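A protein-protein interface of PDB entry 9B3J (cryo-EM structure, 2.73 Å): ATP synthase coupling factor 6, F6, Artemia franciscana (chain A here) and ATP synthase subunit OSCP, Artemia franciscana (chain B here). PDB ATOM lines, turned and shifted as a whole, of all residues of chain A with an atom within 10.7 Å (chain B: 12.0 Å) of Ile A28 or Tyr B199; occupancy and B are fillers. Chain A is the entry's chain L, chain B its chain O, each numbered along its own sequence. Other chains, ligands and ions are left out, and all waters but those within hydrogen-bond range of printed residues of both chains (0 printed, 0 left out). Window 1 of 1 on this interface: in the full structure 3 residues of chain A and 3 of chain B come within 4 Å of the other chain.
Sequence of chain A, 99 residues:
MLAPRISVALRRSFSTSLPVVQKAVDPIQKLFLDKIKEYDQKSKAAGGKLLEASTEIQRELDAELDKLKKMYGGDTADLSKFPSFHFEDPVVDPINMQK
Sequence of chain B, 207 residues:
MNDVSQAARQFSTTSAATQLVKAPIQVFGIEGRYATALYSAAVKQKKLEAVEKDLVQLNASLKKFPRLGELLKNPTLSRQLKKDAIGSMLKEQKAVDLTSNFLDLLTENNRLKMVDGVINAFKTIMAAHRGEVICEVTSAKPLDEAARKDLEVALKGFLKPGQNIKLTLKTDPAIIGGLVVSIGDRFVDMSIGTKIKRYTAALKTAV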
ATOM      1  N   ALA A  24      -8.336 -16.202 -18.230  1.00  0.00           N
ATOM      2  CA  ALA A  24      -7.876 -16.077 -19.613  1.00  0.00           C
ATOM      3  C   ALA A  24      -6.497 -15.416 -19.635  1.00  0.00           C
ATOM      4  O   ALA A  24      -6.325 -14.246 -19.979  1.00  0.00           O
ATOM      5  CB  ALA A  24      -8.888 -15.300 -20.443  1.00  0.00           C
ATOM      6  N   VAL A  25      -5.498 -16.207 -19.254  1.00  0.00           N
ATOM      7  CA  VAL A  25      -4.119 -15.736 -19.218  1.00  0.00           C
ATOM      8  C   VAL A  25      -3.571 -15.700 -20.637  1.00  0.00           C
ATOM      9  O   VAL A  25      -3.642 -16.694 -21.368  1.00  0.00           O
ATOM     10  CB  VAL A  25      -3.261 -16.634 -18.312  1.00  0.00           C
ATOM     11  CG1 VAL A  25      -1.829 -16.123 -18.258  1.00  0.00           C
ATOM     12  CG2 VAL A  25      -3.860 -16.704 -16.917  1.00  0.00           C
ATOM     13  N   ASP A  26      -3.034 -14.549 -21.031  1.00  0.00           N
ATOM     14  CA  ASP A  26      -2.454 -14.416 -22.359  1.00  0.00           C
ATOM     15  C   ASP A  26      -1.175 -15.246 -22.459  1.00  0.00           C
ATOM     16  O   ASP A  26      -0.415 -15.332 -21.489  1.00  0.00           O
ATOM     17  CB  ASP A  26      -2.153 -12.950 -22.669  1.00  0.00           C
ATOM     18  CG  ASP A  26      -3.409 -12.107 -22.772  1.00  0.00           C
ATOM     19  OD1 ASP A  26      -4.517 -12.674 -22.675  1.00  0.00           O
ATOM     20  OD2 ASP A  26      -3.288 -10.877 -22.948  1.00  0.00           O
ATOM     21  N   PRO A  27      -0.930 -15.891 -23.604  1.00  0.00           N
ATOM     22  CA  PRO A  27       0.313 -16.666 -23.758  1.00  0.00           C
ATOM     23  C   PRO A  27       1.572 -15.822 -23.701  1.00  0.00           C
ATOM     24  O   PRO A  27       2.611 -16.313 -23.246  1.00  0.00           O
ATOM     25  CB  PRO A  27       0.139 -17.329 -25.131  1.00  0.00           C
ATOM     26  CG  PRO A  27      -0.804 -16.438 -25.859  1.00  0.00           C
ATOM     27  CD  PRO A  27      -1.755 -15.922 -24.822  1.00  0.00           C
ATOM     28  N   ILE A  28       1.510 -14.566 -24.150  1.00  0.00           N
ATOM     29  CA  ILE A  28       2.693 -13.711 -24.130  1.00  0.00           C
ATOM     30  C   ILE A  28       3.057 -13.331 -22.702  1.00  0.00           C
ATOM     31  O   ILE A  28       4.235 -13.332 -22.329  1.00  0.00           O
ATOM     32  CB  ILE A  28       2.465 -12.471 -25.014  1.00  0.00           C
ATOM     33  CG1 ILE A  28       2.242 -12.901 -26.462  1.00  0.00           C
ATOM     34  CG2 ILE A  28       3.649 -11.521 -24.940  1.00  0.00           C
ATOM     35  CD1 ILE A  28       3.394 -13.696 -27.032  1.00  0.00           C
ATOM     36  N   GLN A  29       2.054 -13.011 -21.878  1.00  0.00           N
ATOM     37  CA  GLN A  29       2.316 -12.680 -20.480  1.00  0.00           C
ATOM     38  C   GLN A  29       2.871 -13.878 -19.719  1.00  0.00           C
ATOM     39  O   GLN A  29       3.809 -13.738 -18.924  1.00  0.00           O
ATOM     40  CB  GLN A  29       1.040 -12.168 -19.815  1.00  0.00           C
ATOM     41  CG  GLN A  29       0.498 -10.891 -20.425  1.00  0.00           C
ATOM     42  CD  GLN A  29      -0.697 -10.346 -19.671  1.00  0.00           C
ATOM     43  OE1 GLN A  29      -1.050 -10.842 -18.601  1.00  0.00           O
ATOM     44  NE2 GLN A  29      -1.330  -9.319 -20.226  1.00  0.00           N
ATOM     45  N   LYS A  30       2.307 -15.065 -19.958  1.00  0.00           N
ATOM     46  CA  LYS A  30       2.807 -16.273 -19.307  1.00  0.00           C
ATOM     47  C   LYS A  30       4.218 -16.608 -19.772  1.00  0.00           C
ATOM     48  O   LYS A  30       5.057 -17.030 -18.966  1.00  0.00           O
ATOM     49  CB  LYS A  30       1.859 -17.440 -19.575  1.00  0.00           C
ATOM     50  CG  LYS A  30       2.185 -18.697 -18.789  1.00  0.00           C
ATOM     51  CD  LYS A  30       1.122 -19.761 -18.995  1.00  0.00           C
ATOM     52  CE  LYS A  30       1.408 -20.996 -18.160  1.00  0.00           C
ATOM     53  NZ  LYS A  30       0.347 -22.030 -18.316  1.00  0.00           N
ATOM     54  N   LEU A  31       4.501 -16.419 -21.064  1.00  0.00           N
ATOM     55  CA  LEU A  31       5.848 -16.644 -21.578  1.00  0.00           C
ATOM     56  C   LEU A  31       6.841 -15.653 -20.984  1.00  0.00           C
ATOM     57  O   LEU A  31       7.976 -16.024 -20.659  1.00  0.00           O
ATOM     58  CB  LEU A  31       5.845 -16.556 -23.104  1.00  0.00           C
ATOM     59  CG  LEU A  31       7.156 -16.861 -23.827  1.00  0.00           C
ATOM     60  CD1 LEU A  31       7.662 -18.246 -23.462  1.00  0.00           C
ATOM     61  CD2 LEU A  31       6.964 -16.739 -25.329  1.00  0.00           C
ATOM     62  N   PHE A  32       6.430 -14.391 -20.831  1.00  0.00           N
ATOM     63  CA  PHE A  32       7.290 -13.391 -20.207  1.00  0.00           C
ATOM     64  C   PHE A  32       7.577 -13.736 -18.751  1.00  0.00           C
ATOM     65  O   PHE A  32       8.713 -13.591 -18.283  1.00  0.00           O
ATOM     66  CB  PHE A  32       6.648 -12.008 -20.311  1.00  0.00           C
ATOM     67  CG  PHE A  32       7.182 -11.172 -21.438  1.00  0.00           C
ATOM     68  CD1 PHE A  32       8.349 -10.441 -21.282  1.00  0.00           C
ATOM     69  CD2 PHE A  32       6.516 -11.112 -22.651  1.00  0.00           C
ATOM     70  CE1 PHE A  32       8.843  -9.668 -22.318  1.00  0.00           C
ATOM     71  CE2 PHE A  32       7.006 -10.340 -23.691  1.00  0.00           C
ATOM     72  CZ  PHE A  32       8.170  -9.618 -23.523  1.00  0.00           C
ATOM     73  N   LEU A  33       6.556 -14.201 -18.023  1.00  0.00           N
ATOM     74  CA  LEU A  33       6.760 -14.607 -16.635  1.00  0.00           C
ATOM     75  C   LEU A  33       7.675 -15.823 -16.540  1.00  0.00           C
ATOM     76  O   LEU A  33       8.504 -15.913 -15.624  1.00  0.00           O
ATOM     77  CB  LEU A  33       5.416 -14.895 -15.967  1.00  0.00           C
ATOM     78  CG  LEU A  33       4.504 -13.694 -15.710  1.00  0.00           C
ATOM     79  CD1 LEU A  33       3.240 -14.125 -14.978  1.00  0.00           C
ATOM     80  CD2 LEU A  33       5.238 -12.616 -14.932  1.00  0.00           C
ATOM     81  N   ASP A  34       7.535 -16.767 -17.474  1.00  0.00           N
ATOM     82  CA  ASP A  34       8.409 -17.937 -17.488  1.00  0.00           C
ATOM     83  C   ASP A  34       9.854 -17.552 -17.783  1.00  0.00           C
ATOM     84  O   ASP A  34      10.781 -18.107 -17.183  1.00  0.00           O
ATOM     85  CB  ASP A  34       7.906 -18.955 -18.510  1.00  0.00           C
ATOM     86  CG  ASP A  34       6.589 -19.582 -18.104  1.00  0.00           C
ATOM     87  OD1 ASP A  34       6.065 -19.220 -17.028  1.00  0.00           O
ATOM     88  OD2 ASP A  34       6.073 -20.432 -18.859  1.00  0.00           O
ATOM     89  N   LYS A  35      10.064 -16.601 -18.698  1.00  0.00           N
ATOM     90  CA  LYS A  35      11.422 -16.155 -18.997  1.00  0.00           C
ATOM     91  C   LYS A  35      12.030 -15.391 -17.827  1.00  0.00           C
ATOM     92  O   LYS A  35      13.234 -15.498 -17.571  1.00  0.00           O
ATOM     93  CB  LYS A  35      11.430 -15.295 -20.260  1.00  0.00           C
ATOM     94  CG  LYS A  35      11.091 -16.060 -21.524  1.00  0.00           C
ATOM     95  CD  LYS A  35      11.929 -17.320 -21.652  1.00  0.00           C
ATOM     96  CE  LYS A  35      11.555 -18.104 -22.896  1.00  0.00           C
ATOM     97  NZ  LYS A  35      12.397 -19.319 -23.066  1.00  0.00           N
ATOM     98  N   ILE A  36      11.214 -14.612 -17.113  1.00  0.00           N
ATOM     99  CA  ILE A  36      11.703 -13.905 -15.931  1.00  0.00           C
ATOM    100  C   ILE A  36      12.099 -14.892 -14.837  1.00  0.00           C
ATOM    101  O   ILE A  36      13.154 -14.746 -14.203  1.00  0.00           O
ATOM    102  CB  ILE A  36      10.643 -12.900 -15.448  1.00  0.00           C
ATOM    103  CG1 ILE A  36      10.586 -11.705 -16.398  1.00  0.00           C
ATOM    104  CG2 ILE A  36      10.923 -12.435 -14.027  1.00  0.00           C
ATOM    105  CD1 ILE A  36       9.610 -10.641 -15.977  1.00  0.00           C
ATOM    106  N   ILE B 175       5.593  -7.817 -38.338  1.00  0.00           N
ATOM    107  CA  ILE B 175       4.707  -7.841 -37.180  1.00  0.00           C
ATOM    108  C   ILE B 175       5.053  -9.040 -36.308  1.00  0.00           C
ATOM    109  O   ILE B 175       4.326  -9.356 -35.358  1.00  0.00           O
ATOM    110  CB  ILE B 175       3.229  -7.879 -37.613  1.00  0.00           C
ATOM    111  CG1 ILE B 175       3.076  -7.314 -39.025  1.00  0.00           C
ATOM    112  CG2 ILE B 175       2.366  -7.086 -36.641  1.00  0.00           C
ATOM    113  CD1 ILE B 175       1.659  -7.343 -39.542  1.00  0.00           C
ATOM    114  N   ILE B 176       6.149  -9.726 -36.651  1.00  0.00           N
ATOM    115  CA  ILE B 176       6.696 -10.882 -35.936  1.00  0.00           C
ATOM    116  C   ILE B 176       5.697 -12.034 -35.922  1.00  0.00           C
ATOM    117  O   ILE B 176       5.920 -13.068 -36.561  1.00  0.00           O
ATOM    118  CB  ILE B 176       7.137 -10.512 -34.506  1.00  0.00           C
ATOM    119  CG1 ILE B 176       8.153  -9.369 -34.539  1.00  0.00           C
ATOM    120  CG2 ILE B 176       7.717 -11.724 -33.797  1.00  0.00           C
ATOM    121  CD1 ILE B 176       9.429  -9.709 -35.273  1.00  0.00           C
ATOM    122  N   GLY B 177       4.599 -11.873 -35.189  1.00  0.00           N
ATOM    123  CA  GLY B 177       3.563 -12.883 -35.142  1.00  0.00           C
ATOM    124  C   GLY B 177       2.196 -12.293 -34.872  1.00  0.00           C
ATOM    125  O   GLY B 177       2.032 -11.069 -34.865  1.00  0.00           O
ATOM    126  N   GLY B 178       1.206 -13.150 -34.645  1.00  0.00           N
ATOM    127  CA  GLY B 178      -0.129 -12.685 -34.332  1.00  0.00           C
ATOM    128  C   GLY B 178      -0.965 -12.374 -35.553  1.00  0.00           C
ATOM    129  O   GLY B 178      -0.757 -12.954 -36.623  1.00  0.00           O
ATOM    130  N   LEU B 179      -1.917 -11.456 -35.404  1.00  0.00           N
ATOM    131  CA  LEU B 179      -2.845 -11.133 -36.477  1.00  0.00           C
ATOM    132  C   LEU B 179      -3.314  -9.695 -36.318  1.00  0.00           C
ATOM    133  O   LEU B 179      -3.512  -9.220 -35.197  1.00  0.00           O
ATOM    134  CB  LEU B 179      -4.046 -12.084 -36.469  1.00  0.00           C
ATOM    135  CG  LEU B 179      -4.741 -12.313 -37.808  1.00  0.00           C
ATOM    136  CD1 LEU B 179      -3.786 -12.990 -38.771  1.00  0.00           C
ATOM    137  CD2 LEU B 179      -5.996 -13.148 -37.616  1.00  0.00           C
ATOM    138  N   ASP B 189      -5.773  -4.898 -32.557  1.00  0.00           N
ATOM    139  CA  ASP B 189      -4.347  -5.095 -32.795  1.00  0.00           C
ATOM    140  C   ASP B 189      -3.800  -6.267 -31.987  1.00  0.00           C
ATOM    141  O   ASP B 189      -2.699  -6.203 -31.439  1.00  0.00           O
ATOM    142  CB  ASP B 189      -3.565  -3.822 -32.481  1.00  0.00           C
ATOM    143  CG  ASP B 189      -3.911  -3.241 -31.121  1.00  0.00           C
ATOM    144  OD1 ASP B 189      -4.842  -3.759 -30.468  1.00  0.00           O
ATOM    145  OD2 ASP B 189      -3.253  -2.263 -30.707  1.00  0.00           O
ATOM    146  N   MET B 190      -4.570  -7.352 -31.905  1.00  0.00           N
ATOM    147  CA  MET B 190      -4.174  -8.533 -31.137  1.00  0.00           C
ATOM    148  C   MET B 190      -3.122  -9.306 -31.930  1.00  0.00           C
ATOM    149  O   MET B 190      -3.383 -10.349 -32.536  1.00  0.00           O
ATOM    150  CB  MET B 190      -5.390  -9.395 -30.820  1.00  0.00           C
ATOM    151  CG  MET B 190      -5.135 -10.478 -29.786  1.00  0.00           C
ATOM    152  SD  MET B 190      -6.607 -11.455 -29.435  1.00  0.00           S
ATOM    153  CE  MET B 190      -7.710 -10.192 -28.807  1.00  0.00           C
ATOM    154  N   SER B 191      -1.902  -8.776 -31.919  1.00  0.00           N
ATOM    155  CA  SER B 191      -0.773  -9.390 -32.597  1.00  0.00           C
ATOM    156  C   SER B 191       0.378  -9.542 -31.614  1.00  0.00           C
ATOM    157  O   SER B 191       0.467  -8.824 -30.616  1.00  0.00           O
ATOM    158  CB  SER B 191      -0.323  -8.568 -33.814  1.00  0.00           C
ATOM    159  OG  SER B 191       0.170  -7.300 -33.423  1.00  0.00           O
ATOM    160  N   ILE B 192       1.261 -10.497 -31.913  1.00  0.00           N
ATOM    161  CA  ILE B 192       2.373 -10.796 -31.015  1.00  0.00           C
ATOM    162  C   ILE B 192       3.390  -9.660 -31.017  1.00  0.00           C
ATOM    163  O   ILE B 192       3.923  -9.287 -29.962  1.00  0.00           O
ATOM    164  CB  ILE B 192       3.017 -12.142 -31.404  1.00  0.00           C
ATOM    165  CG1 ILE B 192       1.978 -13.264 -31.364  1.00  0.00           C
ATOM    166  CG2 ILE B 192       4.185 -12.475 -30.488  1.00  0.00           C
ATOM    167  CD1 ILE B 192       1.222 -13.362 -30.058  1.00  0.00           C
ATOM    168  N   GLY B 193       3.666  -9.090 -32.193  1.00  0.00           N
ATOM    169  CA  GLY B 193       4.692  -8.060 -32.294  1.00  0.00           C
ATOM    170  C   GLY B 193       4.345  -6.798 -31.525  1.00  0.00           C
ATOM    171  O   GLY B 193       5.171  -6.261 -30.781  1.00  0.00           O
ATOM    172  N   THR B 194       3.106  -6.324 -31.671  1.00  0.00           N
ATOM    173  CA  THR B 194       2.675  -5.150 -30.919  1.00  0.00           C
ATOM    174  C   THR B 194       2.562  -5.446 -29.428  1.00  0.00           C
ATOM    175  O   THR B 194       2.820  -4.561 -28.601  1.00  0.00           O
ATOM    176  CB  THR B 194       1.338  -4.639 -31.454  1.00  0.00           C
ATOM    177  OG1 THR B 194       0.355  -5.677 -31.355  1.00  0.00           O
ATOM    178  CG2 THR B 194       1.475  -4.209 -32.903  1.00  0.00           C
ATOM    179  N   LYS B 195       2.187  -6.678 -29.071  1.00  0.00           N
ATOM    180  CA  LYS B 195       2.065  -7.051 -27.664  1.00  0.00           C
ATOM    181  C   LYS B 195       3.421  -7.028 -26.968  1.00  0.00           C
ATOM    182  O   LYS B 195       3.565  -6.453 -25.879  1.00  0.00           O
ATOM    183  CB  LYS B 195       1.429  -8.436 -27.546  1.00  0.00           C
ATOM    184  CG  LYS B 195       0.759  -8.705 -26.215  1.00  0.00           C
ATOM    185  CD  LYS B 195      -0.567  -7.977 -26.114  1.00  0.00           C
ATOM    186  CE  LYS B 195      -1.530  -8.452 -27.190  1.00  0.00           C
ATOM    187  NZ  LYS B 195      -2.838  -7.747 -27.123  1.00  0.00           N
ATOM    188  N   ILE B 196       4.437  -7.628 -27.595  1.00  0.00           N
ATOM    189  CA  ILE B 196       5.760  -7.615 -26.983  1.00  0.00           C
ATOM    190  C   ILE B 196       6.379  -6.225 -27.066  1.00  0.00           C
ATOM    191  O   ILE B 196       7.181  -5.851 -26.202  1.00  0.00           O
ATOM    192  CB  ILE B 196       6.672  -8.689 -27.612  1.00  0.00           C
ATOM    193  CG1 ILE B 196       6.960  -8.390 -29.084  1.00  0.00           C
ATOM    194  CG2 ILE B 196       6.049 -10.067 -27.460  1.00  0.00           C
ATOM    195  CD1 ILE B 196       7.883  -9.392 -29.740  1.00  0.00           C
ATOM    196  N   LYS B 197       5.998  -5.424 -28.070  1.00  0.00           N
ATOM    197  CA  LYS B 197       6.518  -4.065 -28.170  1.00  0.00           C
ATOM    198  C   LYS B 197       6.014  -3.191 -27.028  1.00  0.00           C
ATOM    199  O   LYS B 197       6.794  -2.469 -26.394  1.00  0.00           O
ATOM    200  CB  LYS B 197       6.134  -3.459 -29.518  1.00  0.00           C
ATOM    201  CG  LYS B 197       6.607  -2.032 -29.713  1.00  0.00           C
ATOM    202  CD  LYS B 197       6.119  -1.474 -31.037  1.00  0.00           C
ATOM    203  CE  LYS B 197       6.627  -0.061 -31.262  1.00  0.00           C
ATOM    204  NZ  LYS B 197       8.114  -0.013 -31.320  1.00  0.00           N
ATOM    205  N   ARG B 198       4.712  -3.262 -26.735  1.00  0.00           N
ATOM    206  CA  ARG B 198       4.184  -2.466 -25.632  1.00  0.00           C
ATOM    207  C   ARG B 198       4.608  -3.030 -24.281  1.00  0.00           C
ATOM    208  O   ARG B 198       4.742  -2.270 -23.315  1.00  0.00           O
ATOM    209  CB  ARG B 198       2.660  -2.362 -25.716  1.00  0.00           C
ATOM    210  CG  ARG B 198       1.907  -3.668 -25.536  1.00  0.00           C
ATOM    211  CD  ARG B 198       0.415  -3.422 -25.389  1.00  0.00           C
ATOM    212  NE  ARG B 198      -0.101  -2.568 -26.451  1.00  0.00           N
ATOM    213  CZ  ARG B 198      -0.577  -3.012 -27.606  1.00  0.00           C
ATOM    214  NH1 ARG B 198      -0.620  -4.305 -27.886  1.00  0.00           N
ATOM    215  NH2 ARG B 198      -1.021  -2.137 -28.503  1.00  0.00           N
ATOM    216  N   TYR B 199       4.854  -4.343 -24.195  1.00  0.00           N
ATOM    217  CA  TYR B 199       5.353  -4.904 -22.942  1.00  0.00           C
ATOM    218  C   TYR B 199       6.786  -4.461 -22.665  1.00  0.00           C
ATOM    219  O   TYR B 199       7.125  -4.119 -21.527  1.00  0.00           O
ATOM    220  CB  TYR B 199       5.254  -6.428 -22.970  1.00  0.00           C
ATOM    221  CG  TYR B 199       3.842  -6.952 -22.831  1.00  0.00           C
ATOM    222  CD1 TYR B 199       2.807  -6.122 -22.418  1.00  0.00           C
ATOM    223  CD2 TYR B 199       3.545  -8.279 -23.108  1.00  0.00           C
ATOM    224  CE1 TYR B 199       1.518  -6.596 -22.291  1.00  0.00           C
ATOM    225  CE2 TYR B 199       2.257  -8.765 -22.978  1.00  0.00           C
ATOM    226  CZ  TYR B 199       1.249  -7.918 -22.572  1.00  0.00           C
ATOM    227  OH  TYR B 199      -0.037  -8.390 -22.443  1.00  0.00           O
ATOM    228  N   THR B 200       7.638  -4.454 -23.696  1.00  0.00           N
ATOM    229  CA  THR B 200       9.001  -3.963 -23.526  1.00  0.00           C
ATOM    230  C   THR B 200       9.022  -2.465 -23.260  1.00  0.00           C
ATOM    231  O   THR B 200       9.858  -1.980 -22.487  1.00  0.00           O
ATOM    232  CB  THR B 200       9.840  -4.296 -24.758  1.00  0.00           C
ATOM    233  OG1 THR B 200       9.141  -3.885 -25.940  1.00  0.00           O
ATOM    234  CG2 THR B 200      10.113  -5.785 -24.822  1.00  0.00           C
ATOM    235  N   ALA B 201       8.115  -1.714 -23.894  1.00  0.00           N
ATOM    236  CA  ALA B 201       8.010  -0.286 -23.615  1.00  0.00           C
ATOM    237  C   ALA B 201       7.572  -0.035 -22.178  1.00  0.00           C
ATOM    238  O   ALA B 201       8.080   0.879 -21.517  1.00  0.00           O
ATOM    239  CB  ALA B 201       7.039   0.370 -24.596  1.00  0.00           C
ATOM    240  N   ALA B 202       6.634  -0.843 -21.673  1.00  0.00           N
ATOM    241  CA  ALA B 202       6.214  -0.724 -20.280  1.00  0.00           C
ATOM    242  C   ALA B 202       7.346  -1.080 -19.325  1.00  0.00           C
ATOM    243  O   ALA B 202       7.527  -0.417 -18.294  1.00  0.00           O
ATOM    244  CB  ALA B 202       4.995  -1.609 -20.025  1.00  0.00           C
ATOM    245  N   LEU B 203       8.120  -2.121 -19.650  1.00  0.00           N
ATOM    246  CA  LEU B 203       9.235  -2.511 -18.790  1.00  0.00           C
ATOM    247  C   LEU B 203      10.335  -1.457 -18.789  1.00  0.00           C
ATOM    248  O   LEU B 203      10.983  -1.233 -17.761  1.00  0.00           O
ATOM    249  CB  LEU B 203       9.795  -3.864 -19.225  1.00  0.00           C
ATOM    250  CG  LEU B 203       8.918  -5.086 -18.956  1.00  0.00           C
ATOM    251  CD1 LEU B 203       9.665  -6.362 -19.304  1.00  0.00           C
ATOM    252  CD2 LEU B 203       8.443  -5.107 -17.512  1.00  0.00           C
ATOM    253  N   LYS B 204      10.568  -0.805 -19.931  1.00  0.00           N
ATOM    254  CA  LYS B 204      11.587   0.238 -19.983  1.00  0.00           C
ATOM    255  C   LYS B 204      11.131   1.500 -19.262  1.00  0.00           C
ATOM    256  O   LYS B 204      11.925   2.141 -18.564  1.00  0.00           O
ATOM    257  CB  LYS B 204      11.949   0.550 -21.435  1.00  0.00           C
ATOM    258  CG  LYS B 204      12.792  -0.521 -22.106  1.00  0.00           C
ATOM    259  CD  LYS B 204      13.157  -0.130 -23.528  1.00  0.00           C
ATOM    260  CE  LYS B 204      14.041  -1.181 -24.178  1.00  0.00           C
ATOM    261  NZ  LYS B 204      14.416  -0.813 -25.573  1.00  0.00           N
ATOM    262  N   THR B 205       9.857   1.872 -19.409  1.00  0.00           N
ATOM    263  CA  THR B 205       9.362   3.089 -18.782  1.00  0.00           C
ATOM    264  C   THR B 205       9.076   2.923 -17.294  1.00  0.00           C
ATOM    265  O   THR B 205       8.942   3.931 -16.591  1.00  0.00           O
ATOM    266  CB  THR B 205       8.095   3.575 -19.491  1.00  0.00           C
ATOM    267  OG1 THR B 205       7.163   2.494 -19.606  1.00  0.00           O
ATOM    268  CG2 THR B 205       8.430   4.109 -20.878  1.00  0.00           C
ATOM    269  N   ALA B 206       8.975   1.689 -16.798  1.00  0.00           N
ATOM    270  CA  ALA B 206       8.731   1.447 -15.382  1.00  0.00           C
ATOM    271  C   ALA B 206       9.953   0.922 -14.643  1.00  0.00           C
ATOM    272  O   ALA B 206      10.283   1.418 -13.562  1.00  0.00           O
ATOM    273  CB  ALA B 206       7.561   0.469 -15.210  1.00  0.00           C
ATOM    274  N   VAL B 207      10.631  -0.079 -15.196  1.00  0.00           N
ATOM    275  CA  VAL B 207      11.798  -0.675 -14.550  1.00  0.00           C
ATOM    276  C   VAL B 207      13.032  -0.317 -15.391  1.00  0.00           C
ATOM    277  O   VAL B 207      12.899   0.366 -16.405  1.00  0.00           O
ATOM    278  CB  VAL B 207      11.599  -2.209 -14.372  1.00  0.00           C
ATOM    279  CG1 VAL B 207      12.669  -2.830 -13.475  1.00  0.00           C
ATOM    280  CG2 VAL B 207      10.223  -2.490 -13.784  1.00  0.00           C
ATOM    281  OXT VAL B 207      14.190  -0.631 -15.108  1.00  0.00           O
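OH of Tyr B199 lies within hydrogen-bond range of NE2 of Gln A29 (2.7 Å).
The backbone carbonyl oxygen (O) of Gly B177 sits at hydrogen-bond distance from the backbone NH (N) of Ile B192, at 3.1 Å. O of Ile B196 lies within hydrogen-bond range of OG1 of Thr B200.
Ile B192 touches Ile A28. Ile B196 touches Ile A28 (CG2 to CG2, 3.8 Å). CG2 of Ile A28 touches CE2 of Tyr B199 (3.7 Å). Phe A32 touches Ile B196.
Ile A28 touches just these residues of chain B: Ile B192 (3.7 Å), Ile B196 (3.8 Å) and Tyr B199 (3.7 Å). Of chain A, only Ile A28 (3.7 Å) and Gln A29 (2.7 Å) come within 4 Å of Tyr B199. Asp A26 touches none of the printed residues of chain B. Of the printed residues of chain B, Gln A29 touches Tyr B199 (2.7 Å). Of chain B, only Ile B196 comes within 4 Å of Phe A32. No residue of chain A comes within 4 Å of Ala B202. No residue of chain A comes within 4 Å of Leu B203. Of the printed residues of chain A, Ile B196 touches Ile A28 and Phe A32. Gly B178 touches none of the printed residues of chain A. The nearest printed residue of chain A that does not touch Ile B196 is Leu A31 (7.1 Å).
Hydrophobic or aromatic side chains of chain A that line the printed part of chain B: Ile A28 and Phe A32. Among the printed residues, 5 pairs touch across the chains. Among the printed residues, no Asp or Glu carboxylate lies within 4 Å of a Lys or Arg side-chain nitrogen of the other chain.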
